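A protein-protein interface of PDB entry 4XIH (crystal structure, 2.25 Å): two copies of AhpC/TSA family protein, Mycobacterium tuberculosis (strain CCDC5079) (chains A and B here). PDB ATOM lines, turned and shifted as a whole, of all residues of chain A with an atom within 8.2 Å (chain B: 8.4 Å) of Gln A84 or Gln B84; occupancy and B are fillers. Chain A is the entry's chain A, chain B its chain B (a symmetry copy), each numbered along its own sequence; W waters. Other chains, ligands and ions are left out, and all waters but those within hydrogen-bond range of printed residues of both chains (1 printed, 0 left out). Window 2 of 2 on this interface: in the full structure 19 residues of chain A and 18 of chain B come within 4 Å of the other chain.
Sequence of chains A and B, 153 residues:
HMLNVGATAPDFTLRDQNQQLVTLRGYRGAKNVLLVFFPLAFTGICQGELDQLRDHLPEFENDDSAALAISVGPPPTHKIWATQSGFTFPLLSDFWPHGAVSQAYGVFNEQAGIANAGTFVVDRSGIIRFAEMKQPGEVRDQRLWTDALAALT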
ATOM      1  N   PHE A  42      10.879 -22.300  10.321  1.00  0.00           N
ATOM      2  CA  PHE A  42      11.035 -23.682   9.844  1.00  0.00           C
ATOM      3  C   PHE A  42       9.769 -24.541   9.875  1.00  0.00           C
ATOM      4  O   PHE A  42       9.849 -25.759   9.712  1.00  0.00           O
ATOM      5  CB  PHE A  42      12.146 -24.412  10.606  1.00  0.00           C
ATOM      6  CG  PHE A  42      13.453 -23.680  10.626  1.00  0.00           C
ATOM      7  CD1 PHE A  42      14.150 -23.450   9.448  1.00  0.00           C
ATOM      8  CD2 PHE A  42      14.011 -23.262  11.825  1.00  0.00           C
ATOM      9  CE1 PHE A  42      15.367 -22.790   9.462  1.00  0.00           C
ATOM     10  CE2 PHE A  42      15.229 -22.604  11.846  1.00  0.00           C
ATOM     11  CZ  PHE A  42      15.908 -22.368  10.664  1.00  0.00           C
ATOM     12  N   GLN A  47       6.109 -20.726   6.802  1.00  0.00           N
ATOM     13  CA  GLN A  47       6.838 -20.662   5.546  1.00  0.00           C
ATOM     14  C   GLN A  47       5.899 -20.140   4.468  1.00  0.00           C
ATOM     15  O   GLN A  47       6.244 -19.219   3.734  1.00  0.00           O
ATOM     16  CB  GLN A  47       7.359 -22.048   5.151  1.00  0.00           C
ATOM     17  CG  GLN A  47       8.301 -22.048   3.956  1.00  0.00           C
ATOM     18  CD  GLN A  47       9.679 -21.515   4.298  1.00  0.00           C
ATOM     19  OE1 GLN A  47      10.333 -22.012   5.213  1.00  0.00           O
ATOM     20  NE2 GLN A  47      10.136 -20.520   3.550  1.00  0.00           N
ATOM     21  N   ASP A  51       6.533 -16.648   2.664  1.00  0.00           N
ATOM     22  CA  ASP A  51       6.823 -16.809   1.238  1.00  0.00           C
ATOM     23  C   ASP A  51       5.900 -15.895   0.440  1.00  0.00           C
ATOM     24  O   ASP A  51       6.328 -15.249  -0.513  1.00  0.00           O
ATOM     25  CB  ASP A  51       6.639 -18.258   0.775  1.00  0.00           C
ATOM     26  CG  ASP A  51       7.762 -19.180   1.235  1.00  0.00           C
ATOM     27  OD1 ASP A  51       8.652 -18.740   1.997  1.00  0.00           O
ATOM     28  OD2 ASP A  51       7.751 -20.361   0.822  1.00  0.00           O
ATOM     29  N   ARG A  54       7.254 -12.543   0.865  1.00  0.00           N
ATOM     30  CA  ARG A  54       8.464 -12.442   0.047  1.00  0.00           C
ATOM     31  C   ARG A  54       8.137 -12.258  -1.430  1.00  0.00           C
ATOM     32  O   ARG A  54       8.734 -11.416  -2.105  1.00  0.00           O
ATOM     33  CB  ARG A  54       9.309 -13.713   0.207  1.00  0.00           C
ATOM     34  CG  ARG A  54      10.531 -13.815  -0.710  1.00  0.00           C
ATOM     35  CD  ARG A  54      11.044 -15.247  -0.769  1.00  0.00           C
ATOM     36  NE  ARG A  54      10.028 -16.134  -1.333  1.00  0.00           N
ATOM     37  CZ  ARG A  54      10.087 -17.464  -1.354  1.00  0.00           C
ATOM     38  NH1 ARG A  54      11.123 -18.118  -0.834  1.00  0.00           N
ATOM     39  NH2 ARG A  54       9.087 -18.150  -1.896  1.00  0.00           N
ATOM     40  N   THR A  77      18.542 -18.128  14.399  1.00  0.00           N
ATOM     41  CA  THR A  77      17.479 -18.938  13.828  1.00  0.00           C
ATOM     42  C   THR A  77      16.892 -18.245  12.609  1.00  0.00           C
ATOM     43  O   THR A  77      16.774 -18.849  11.543  1.00  0.00           O
ATOM     44  CB  THR A  77      16.356 -19.159  14.856  1.00  0.00           C
ATOM     45  OG1 THR A  77      16.856 -19.953  15.938  1.00  0.00           O
ATOM     46  CG2 THR A  77      15.150 -19.847  14.226  1.00  0.00           C
ATOM     47  N   HIS A  78      16.525 -16.976  12.775  1.00  0.00           N
ATOM     48  CA  HIS A  78      15.949 -16.206  11.677  1.00  0.00           C
ATOM     49  C   HIS A  78      16.946 -15.984  10.557  1.00  0.00           C
ATOM     50  O   HIS A  78      16.562 -15.930   9.394  1.00  0.00           O
ATOM     51  CB  HIS A  78      15.433 -14.846  12.138  1.00  0.00           C
ATOM     52  CG  HIS A  78      14.264 -14.925  13.062  1.00  0.00           C
ATOM     53  ND1 HIS A  78      14.098 -14.066  14.125  1.00  0.00           N
ATOM     54  CD2 HIS A  78      13.213 -15.776  13.097  1.00  0.00           C
ATOM     55  CE1 HIS A  78      12.979 -14.367  14.759  1.00  0.00           C
ATOM     56  NE2 HIS A  78      12.427 -15.406  14.159  1.00  0.00           N
ATOM     57  N   LYS A  79      18.217 -15.834  10.914  1.00  0.00           N
ATOM     58  CA  LYS A  79      19.260 -15.625   9.928  1.00  0.00           C
ATOM     59  C   LYS A  79      19.322 -16.802   8.969  1.00  0.00           C
ATOM     60  O   LYS A  79      19.205 -16.631   7.755  1.00  0.00           O
ATOM     61  CB  LYS A  79      20.611 -15.417  10.615  1.00  0.00           C
ATOM     62  CG  LYS A  79      21.780 -15.191   9.665  1.00  0.00           C
ATOM     63  CD  LYS A  79      21.460 -14.104   8.651  1.00  0.00           C
ATOM     64  CE  LYS A  79      22.674 -13.710   7.828  1.00  0.00           C
ATOM     65  NZ  LYS A  79      22.310 -12.678   6.815  1.00  0.00           N
ATOM     66  N   ILE A  80      19.480 -17.995   9.531  1.00  0.00           N
ATOM     67  CA  ILE A  80      19.561 -19.223   8.743  1.00  0.00           C
ATOM     68  C   ILE A  80      18.299 -19.432   7.906  1.00  0.00           C
ATOM     69  O   ILE A  80      18.381 -19.762   6.722  1.00  0.00           O
ATOM     70  CB  ILE A  80      19.800 -20.451   9.656  1.00  0.00           C
ATOM     71  CG1 ILE A  80      21.206 -20.399  10.273  1.00  0.00           C
ATOM     72  CG2 ILE A  80      19.632 -21.759   8.887  1.00  0.00           C
ATOM     73  CD1 ILE A  80      22.344 -20.634   9.293  1.00  0.00           C
ATOM     74  N   TRP A  81      17.141 -19.226   8.522  1.00  0.00           N
ATOM     75  CA  TRP A  81      15.866 -19.422   7.839  1.00  0.00           C
ATOM     76  C   TRP A  81      15.668 -18.416   6.707  1.00  0.00           C
ATOM     77  O   TRP A  81      15.152 -18.768   5.647  1.00  0.00           O
ATOM     78  CB  TRP A  81      14.711 -19.362   8.841  1.00  0.00           C
ATOM     79  CG  TRP A  81      13.395 -19.793   8.276  1.00  0.00           C
ATOM     80  CD1 TRP A  81      13.151 -20.902   7.519  1.00  0.00           C
ATOM     81  CD2 TRP A  81      12.122 -19.174   8.497  1.00  0.00           C
ATOM     82  NE1 TRP A  81      11.816 -20.988   7.217  1.00  0.00           N
ATOM     83  CE2 TRP A  81      11.160 -19.939   7.804  1.00  0.00           C
ATOM     84  CE3 TRP A  81      11.704 -18.034   9.194  1.00  0.00           C
ATOM     85  CZ2 TRP A  81       9.804 -19.606   7.797  1.00  0.00           C
ATOM     86  CZ3 TRP A  81      10.360 -17.704   9.183  1.00  0.00           C
ATOM     87  CH2 TRP A  81       9.425 -18.487   8.488  1.00  0.00           C
ATOM     88  N   ALA A  82      16.091 -17.174   6.936  1.00  0.00           N
ATOM     89  CA  ALA A  82      15.988 -16.120   5.928  1.00  0.00           C
ATOM     90  C   ALA A  82      16.878 -16.432   4.730  1.00  0.00           C
ATOM     91  O   ALA A  82      16.492 -16.200   3.585  1.00  0.00           O
ATOM     92  CB  ALA A  82      16.361 -14.772   6.526  1.00  0.00           C
ATOM     93  N   THR A  83      18.069 -16.955   5.009  1.00  0.00           N
ATOM     94  CA  THR A  83      19.029 -17.340   3.978  1.00  0.00           C
ATOM     95  C   THR A  83      18.488 -18.498   3.132  1.00  0.00           C
ATOM     96  O   THR A  83      18.635 -18.496   1.911  1.00  0.00           O
ATOM     97  CB  THR A  83      20.377 -17.739   4.614  1.00  0.00           C
ATOM     98  OG1 THR A  83      20.904 -16.630   5.354  1.00  0.00           O
ATOM     99  CG2 THR A  83      21.390 -18.167   3.554  1.00  0.00           C
ATOM    100  N   GLN A  84      17.871 -19.480   3.790  1.00  0.00           N
ATOM    101  CA  GLN A  84      17.282 -20.634   3.102  1.00  0.00           C
ATOM    102  C   GLN A  84      16.017 -20.297   2.324  1.00  0.00           C
ATOM    103  O   GLN A  84      15.742 -20.916   1.301  1.00  0.00           O
ATOM    104  CB  GLN A  84      16.932 -21.749   4.088  1.00  0.00           C
ATOM    105  CG  GLN A  84      18.123 -22.501   4.651  1.00  0.00           C
ATOM    106  CD  GLN A  84      17.709 -23.594   5.623  1.00  0.00           C
ATOM    107  OE1 GLN A  84      16.544 -23.684   6.027  1.00  0.00           O
ATOM    108  NE2 GLN A  84      18.665 -24.426   6.010  1.00  0.00           N
ATOM    109  N   SER A  85      15.241 -19.341   2.824  1.00  0.00           N
ATOM    110  CA  SER A  85      13.986 -18.959   2.187  1.00  0.00           C
ATOM    111  C   SER A  85      14.101 -17.733   1.283  1.00  0.00           C
ATOM    112  O   SER A  85      13.162 -17.412   0.557  1.00  0.00           O
ATOM    113  CB  SER A  85      12.934 -18.695   3.258  1.00  0.00           C
ATOM    114  OG  SER A  85      12.731 -19.843   4.063  1.00  0.00           O
ATOM    115  N   GLY A  86      15.239 -17.051   1.327  1.00  0.00           N
ATOM    116  CA  GLY A  86      15.436 -15.851   0.524  1.00  0.00           C
ATOM    117  C   GLY A  86      14.656 -14.653   1.043  1.00  0.00           C
ATOM    118  O   GLY A  86      14.157 -13.853   0.250  1.00  0.00           O
ATOM    119  N   PHE A  87      14.536 -14.533   2.367  1.00  0.00           N
ATOM    120  CA  PHE A  87      13.851 -13.390   2.973  1.00  0.00           C
ATOM    121  C   PHE A  87      14.842 -12.242   3.143  1.00  0.00           C
ATOM    122  O   PHE A  87      15.867 -12.401   3.807  1.00  0.00           O
ATOM    123  CB  PHE A  87      13.255 -13.722   4.351  1.00  0.00           C
ATOM    124  CG  PHE A  87      12.294 -14.884   4.361  1.00  0.00           C
ATOM    125  CD1 PHE A  87      11.365 -15.068   3.344  1.00  0.00           C
ATOM    126  CD2 PHE A  87      12.257 -15.743   5.452  1.00  0.00           C
ATOM    127  CE1 PHE A  87      10.468 -16.123   3.384  1.00  0.00           C
ATOM    128  CE2 PHE A  87      11.354 -16.791   5.504  1.00  0.00           C
ATOM    129  CZ  PHE A  87      10.458 -16.981   4.468  1.00  0.00           C
ATOM    130  N   PHE B  42      22.711 -22.974  15.701  1.00  0.00           N
ATOM    131  CA  PHE B  42      23.265 -22.139  14.627  1.00  0.00           C
ATOM    132  C   PHE B  42      24.318 -21.130  15.088  1.00  0.00           C
ATOM    133  O   PHE B  42      24.511 -20.098  14.445  1.00  0.00           O
ATOM    134  CB  PHE B  42      22.155 -21.427  13.847  1.00  0.00           C
ATOM    135  CG  PHE B  42      21.051 -22.341  13.396  1.00  0.00           C
ATOM    136  CD1 PHE B  42      21.305 -23.350  12.475  1.00  0.00           C
ATOM    137  CD2 PHE B  42      19.757 -22.176  13.865  1.00  0.00           C
ATOM    138  CE1 PHE B  42      20.290 -24.188  12.045  1.00  0.00           C
ATOM    139  CE2 PHE B  42      18.738 -23.012  13.437  1.00  0.00           C
ATOM    140  CZ  PHE B  42      19.005 -24.019  12.529  1.00  0.00           C
ATOM    141  N   GLN B  47      27.896 -25.433  17.797  1.00  0.00           N
ATOM    142  CA  GLN B  47      28.134 -26.298  16.654  1.00  0.00           C
ATOM    143  C   GLN B  47      29.342 -27.186  16.937  1.00  0.00           C
ATOM    144  O   GLN B  47      29.265 -28.408  16.836  1.00  0.00           O
ATOM    145  CB  GLN B  47      28.388 -25.458  15.397  1.00  0.00           C
ATOM    146  CG  GLN B  47      28.431 -26.262  14.112  1.00  0.00           C
ATOM    147  CD  GLN B  47      27.062 -26.764  13.710  1.00  0.00           C
ATOM    148  OE1 GLN B  47      26.155 -25.973  13.457  1.00  0.00           O
ATOM    149  NE2 GLN B  47      26.910 -28.080  13.630  1.00  0.00           N
ATOM    150  N   ASP B  51      29.194 -31.056  17.395  1.00  0.00           N
ATOM    151  CA  ASP B  51      29.897 -31.777  16.321  1.00  0.00           C
ATOM    152  C   ASP B  51      30.846 -32.800  16.933  1.00  0.00           C
ATOM    153  O   ASP B  51      30.950 -33.921  16.445  1.00  0.00           O
ATOM    154  CB  ASP B  51      30.703 -30.834  15.412  1.00  0.00           C
ATOM    155  CG  ASP B  51      29.840 -30.085  14.410  1.00  0.00           C
ATOM    156  OD1 ASP B  51      28.613 -30.331  14.355  1.00  0.00           O
ATOM    157  OD2 ASP B  51      30.401 -29.250  13.662  1.00  0.00           O
ATOM    158  N   ARG B  54      28.807 -35.588  18.239  1.00  0.00           N
ATOM    159  CA  ARG B  54      28.398 -36.391  17.084  1.00  0.00           C
ATOM    160  C   ARG B  54      29.524 -37.341  16.654  1.00  0.00           C
ATOM    161  O   ARG B  54      29.283 -38.519  16.379  1.00  0.00           O
ATOM    162  CB  ARG B  54      28.048 -35.458  15.923  1.00  0.00           C
ATOM    163  CG  ARG B  54      27.795 -36.122  14.575  1.00  0.00           C
ATOM    164  CD  ARG B  54      27.887 -35.077  13.473  1.00  0.00           C
ATOM    165  NE  ARG B  54      29.247 -34.538  13.378  1.00  0.00           N
ATOM    166  CZ  ARG B  54      29.591 -33.432  12.722  1.00  0.00           C
ATOM    167  NH1 ARG B  54      28.679 -32.696  12.095  1.00  0.00           N
ATOM    168  NH2 ARG B  54      30.858 -33.046  12.711  1.00  0.00           N
ATOM    169  N   THR B  77      13.361 -25.835  15.165  1.00  0.00           N
ATOM    170  CA  THR B  77      14.710 -25.299  15.119  1.00  0.00           C
ATOM    171  C   THR B  77      15.720 -26.434  15.265  1.00  0.00           C
ATOM    172  O   THR B  77      16.646 -26.547  14.460  1.00  0.00           O
ATOM    173  CB  THR B  77      14.935 -24.251  16.224  1.00  0.00           C
ATOM    174  OG1 THR B  77      14.144 -23.091  15.938  1.00  0.00           O
ATOM    175  CG2 THR B  77      16.409 -23.850  16.323  1.00  0.00           C
ATOM    176  N   HIS B  78      15.533 -27.277  16.278  1.00  0.00           N
ATOM    177  CA  HIS B  78      16.449 -28.397  16.499  1.00  0.00           C
ATOM    178  C   HIS B  78      16.402 -29.433  15.385  1.00  0.00           C
ATOM    179  O   HIS B  78      17.423 -30.046  15.078  1.00  0.00           O
ATOM    180  CB  HIS B  78      16.208 -29.083  17.845  1.00  0.00           C
ATOM    181  CG  HIS B  78      16.461 -28.202  19.026  1.00  0.00           C
ATOM    182  ND1 HIS B  78      15.807 -28.362  20.228  1.00  0.00           N
ATOM    183  CD2 HIS B  78      17.261 -27.120  19.173  1.00  0.00           C
ATOM    184  CE1 HIS B  78      16.227 -27.444  21.079  1.00  0.00           C
ATOM    185  NE2 HIS B  78      17.100 -26.671  20.461  1.00  0.00           N
ATOM    186  N   LYS B  79      15.229 -29.630  14.788  1.00  0.00           N
ATOM    187  CA  LYS B  79      15.074 -30.583  13.687  1.00  0.00           C
ATOM    188  C   LYS B  79      15.938 -30.188  12.494  1.00  0.00           C
ATOM    189  O   LYS B  79      16.705 -31.005  11.981  1.00  0.00           O
ATOM    190  CB  LYS B  79      13.604 -30.673  13.265  1.00  0.00           C
ATOM    191  CG  LYS B  79      13.314 -31.600  12.093  1.00  0.00           C
ATOM    192  CD  LYS B  79      13.772 -33.024  12.359  1.00  0.00           C
ATOM    193  CE  LYS B  79      13.319 -33.971  11.258  1.00  0.00           C
ATOM    194  NZ  LYS B  79      13.762 -35.371  11.525  1.00  0.00           N
ATOM    195  N   ILE B  80      15.815 -28.934  12.070  1.00  0.00           N
ATOM    196  CA  ILE B  80      16.581 -28.434  10.928  1.00  0.00           C
ATOM    197  C   ILE B  80      18.073 -28.460  11.225  1.00  0.00           C
ATOM    198  O   ILE B  80      18.865 -28.891  10.388  1.00  0.00           O
ATOM    199  CB  ILE B  80      16.161 -26.998  10.538  1.00  0.00           C
ATOM    200  CG1 ILE B  80      14.690 -26.966  10.092  1.00  0.00           C
ATOM    201  CG2 ILE B  80      17.055 -26.450   9.428  1.00  0.00           C
ATOM    202  CD1 ILE B  80      14.357 -27.861   8.911  1.00  0.00           C
ATOM    203  N   TRP B  81      18.451 -28.012  12.419  1.00  0.00           N
ATOM    204  CA  TRP B  81      19.855 -27.961  12.798  1.00  0.00           C
ATOM    205  C   TRP B  81      20.451 -29.362  12.885  1.00  0.00           C
ATOM    206  O   TRP B  81      21.551 -29.597  12.390  1.00  0.00           O
ATOM    207  CB  TRP B  81      20.034 -27.202  14.113  1.00  0.00           C
ATOM    208  CG  TRP B  81      21.457 -26.858  14.426  1.00  0.00           C
ATOM    209  CD1 TRP B  81      22.388 -26.351  13.559  1.00  0.00           C
ATOM    210  CD2 TRP B  81      22.092 -26.901  15.709  1.00  0.00           C
ATOM    211  NE1 TRP B  81      23.572 -26.122  14.213  1.00  0.00           N
ATOM    212  CE2 TRP B  81      23.419 -26.447  15.534  1.00  0.00           C
ATOM    213  CE3 TRP B  81      21.679 -27.301  16.984  1.00  0.00           C
ATOM    214  CZ2 TRP B  81      24.333 -26.378  16.588  1.00  0.00           C
ATOM    215  CZ3 TRP B  81      22.591 -27.232  18.032  1.00  0.00           C
ATOM    216  CH2 TRP B  81      23.902 -26.774  17.826  1.00  0.00           C
ATOM    217  N   ALA B  82      19.713 -30.288  13.498  1.00  0.00           N
ATOM    218  CA  ALA B  82      20.156 -31.675  13.628  1.00  0.00           C
ATOM    219  C   ALA B  82      20.355 -32.333  12.264  1.00  0.00           C
ATOM    220  O   ALA B  82      21.345 -33.026  12.048  1.00  0.00           O
ATOM    221  CB  ALA B  82      19.161 -32.476  14.457  1.00  0.00           C
ATOM    222  N   THR B  83      19.413 -32.104  11.351  1.00  0.00           N
ATOM    223  CA  THR B  83      19.484 -32.656   9.997  1.00  0.00           C
ATOM    224  C   THR B  83      20.734 -32.174   9.253  1.00  0.00           C
ATOM    225  O   THR B  83      21.481 -32.983   8.711  1.00  0.00           O
ATOM    226  CB  THR B  83      18.217 -32.299   9.192  1.00  0.00           C
ATOM    227  OG1 THR B  83      17.080 -32.896   9.820  1.00  0.00           O
ATOM    228  CG2 THR B  83      18.307 -32.801   7.754  1.00  0.00           C
ATOM    229  N   GLN B  84      20.960 -30.864   9.241  1.00  0.00           N
ATOM    230  CA  GLN B  84      22.130 -30.283   8.572  1.00  0.00           C
ATOM    231  C   GLN B  84      23.448 -30.693   9.230  1.00  0.00           C
ATOM    232  O   GLN B  84      24.442 -30.948   8.546  1.00  0.00           O
ATOM    233  CB  GLN B  84      22.049 -28.753   8.581  1.00  0.00           C
ATOM    234  CG  GLN B  84      20.912 -28.161   7.760  1.00  0.00           C
ATOM    235  CD  GLN B  84      20.869 -26.641   7.824  1.00  0.00           C
ATOM    236  OE1 GLN B  84      20.213 -25.997   7.008  1.00  0.00           O
ATOM    237  NE2 GLN B  84      21.574 -26.058   8.794  1.00  0.00           N
ATOM    238  N   SER B  85      23.450 -30.744  10.558  1.00  0.00           N
ATOM    239  CA  SER B  85      24.648 -31.079  11.318  1.00  0.00           C
ATOM    240  C   SER B  85      24.893 -32.578  11.440  1.00  0.00           C
ATOM    241  O   SER B  85      25.988 -32.996  11.803  1.00  0.00           O
ATOM    242  CB  SER B  85      24.543 -30.494  12.723  1.00  0.00           C
ATOM    243  OG  SER B  85      24.311 -29.102  12.685  1.00  0.00           O
ATOM    244  N   GLY B  86      23.876 -33.381  11.143  1.00  0.00           N
ATOM    245  CA  GLY B  86      23.978 -34.827  11.268  1.00  0.00           C
ATOM    246  C   GLY B  86      23.877 -35.303  12.709  1.00  0.00           C
ATOM    247  O   GLY B  86      24.521 -36.287  13.080  1.00  0.00           O
ATOM    248  N   PHE B  87      23.094 -34.605  13.534  1.00  0.00           N
ATOM    249  CA  PHE B  87      22.907 -35.021  14.927  1.00  0.00           C
ATOM    250  C   PHE B  87      21.765 -36.026  14.982  1.00  0.00           C
ATOM    251  O   PHE B  87      20.655 -35.725  14.547  1.00  0.00           O
ATOM    252  CB  PHE B  87      22.573 -33.850  15.858  1.00  0.00           C
ATOM    253  CG  PHE B  87      23.559 -32.713  15.825  1.00  0.00           C
ATOM    254  CD1 PHE B  87      24.926 -32.944  15.761  1.00  0.00           C
ATOM    255  CD2 PHE B  87      23.115 -31.403  15.951  1.00  0.00           C
ATOM    256  CE1 PHE B  87      25.824 -31.891  15.758  1.00  0.00           C
ATOM    257  CE2 PHE B  87      24.008 -30.346  15.961  1.00  0.00           C
ATOM    258  CZ  PHE B  87      25.368 -30.589  15.866  1.00  0.00           C
HETATM  259  O   HOH W   1      14.899 -21.013  17.499  1.00  0.00           O
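Phe A42 touches its own counterpart, Phe B42. Phe A42 touches Thr B77, and with the chains exchanged Thr A77 touches Phe B42. Phe A42 touches Ile B80, and with the chains exchanged Ile A80 touches Phe B42. Thr A77 touches its own counterpart, Thr B77.
Of the 15 printed residues of chain A, 4 touch a printed residue of chain B. Hydrophobic or aromatic side chains of chain A that line the printed part of chain B: Phe A42 and Ile A80. Of the 15 printed residues of chain B, 4 touch a printed residue of chain A. Hydrophobic or aromatic side chains of chain B within 4 Å of the printed part of chain A: Phe B42 and Ile B80.
NE2 of Gln A84 lies within hydrogen-bond range of OE1 of Gln B84.
Of the printed residues of chain B, Gln A84 touches Gln B84 (2.4 Å). Gln B84 touches one residue of chain A. Of the printed residues of chain B, Thr A77 touches Phe B42 (3.96 Å) and Thr B77 (3.8 Å). Of the printed residues of chain A, Ile B80 touches Phe A42 (3.6 Å). Of the printed residues of chain B, Phe A42 touches Phe B42, Thr B77 and Ile B80. Ser A85 touches none of the printed residues of chain B. The nearest printed residue of chain B that does not touch Phe A42 is His B78 (6.2 Å).
Among the printed residues, merely in contact across the chains: Phe A42 with Phe B42, Phe A42 with Thr B77, Phe A42 with Ile B80, Thr A77 with Phe B42, Thr A77 with Thr B77 and Ile A80 with Phe B42.
Water W1 lies within hydrogen-bond range of the side-chain hydroxyl (OG1) of Thr B77 and the side-chain hydroxyl (OG1) of Thr A77.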
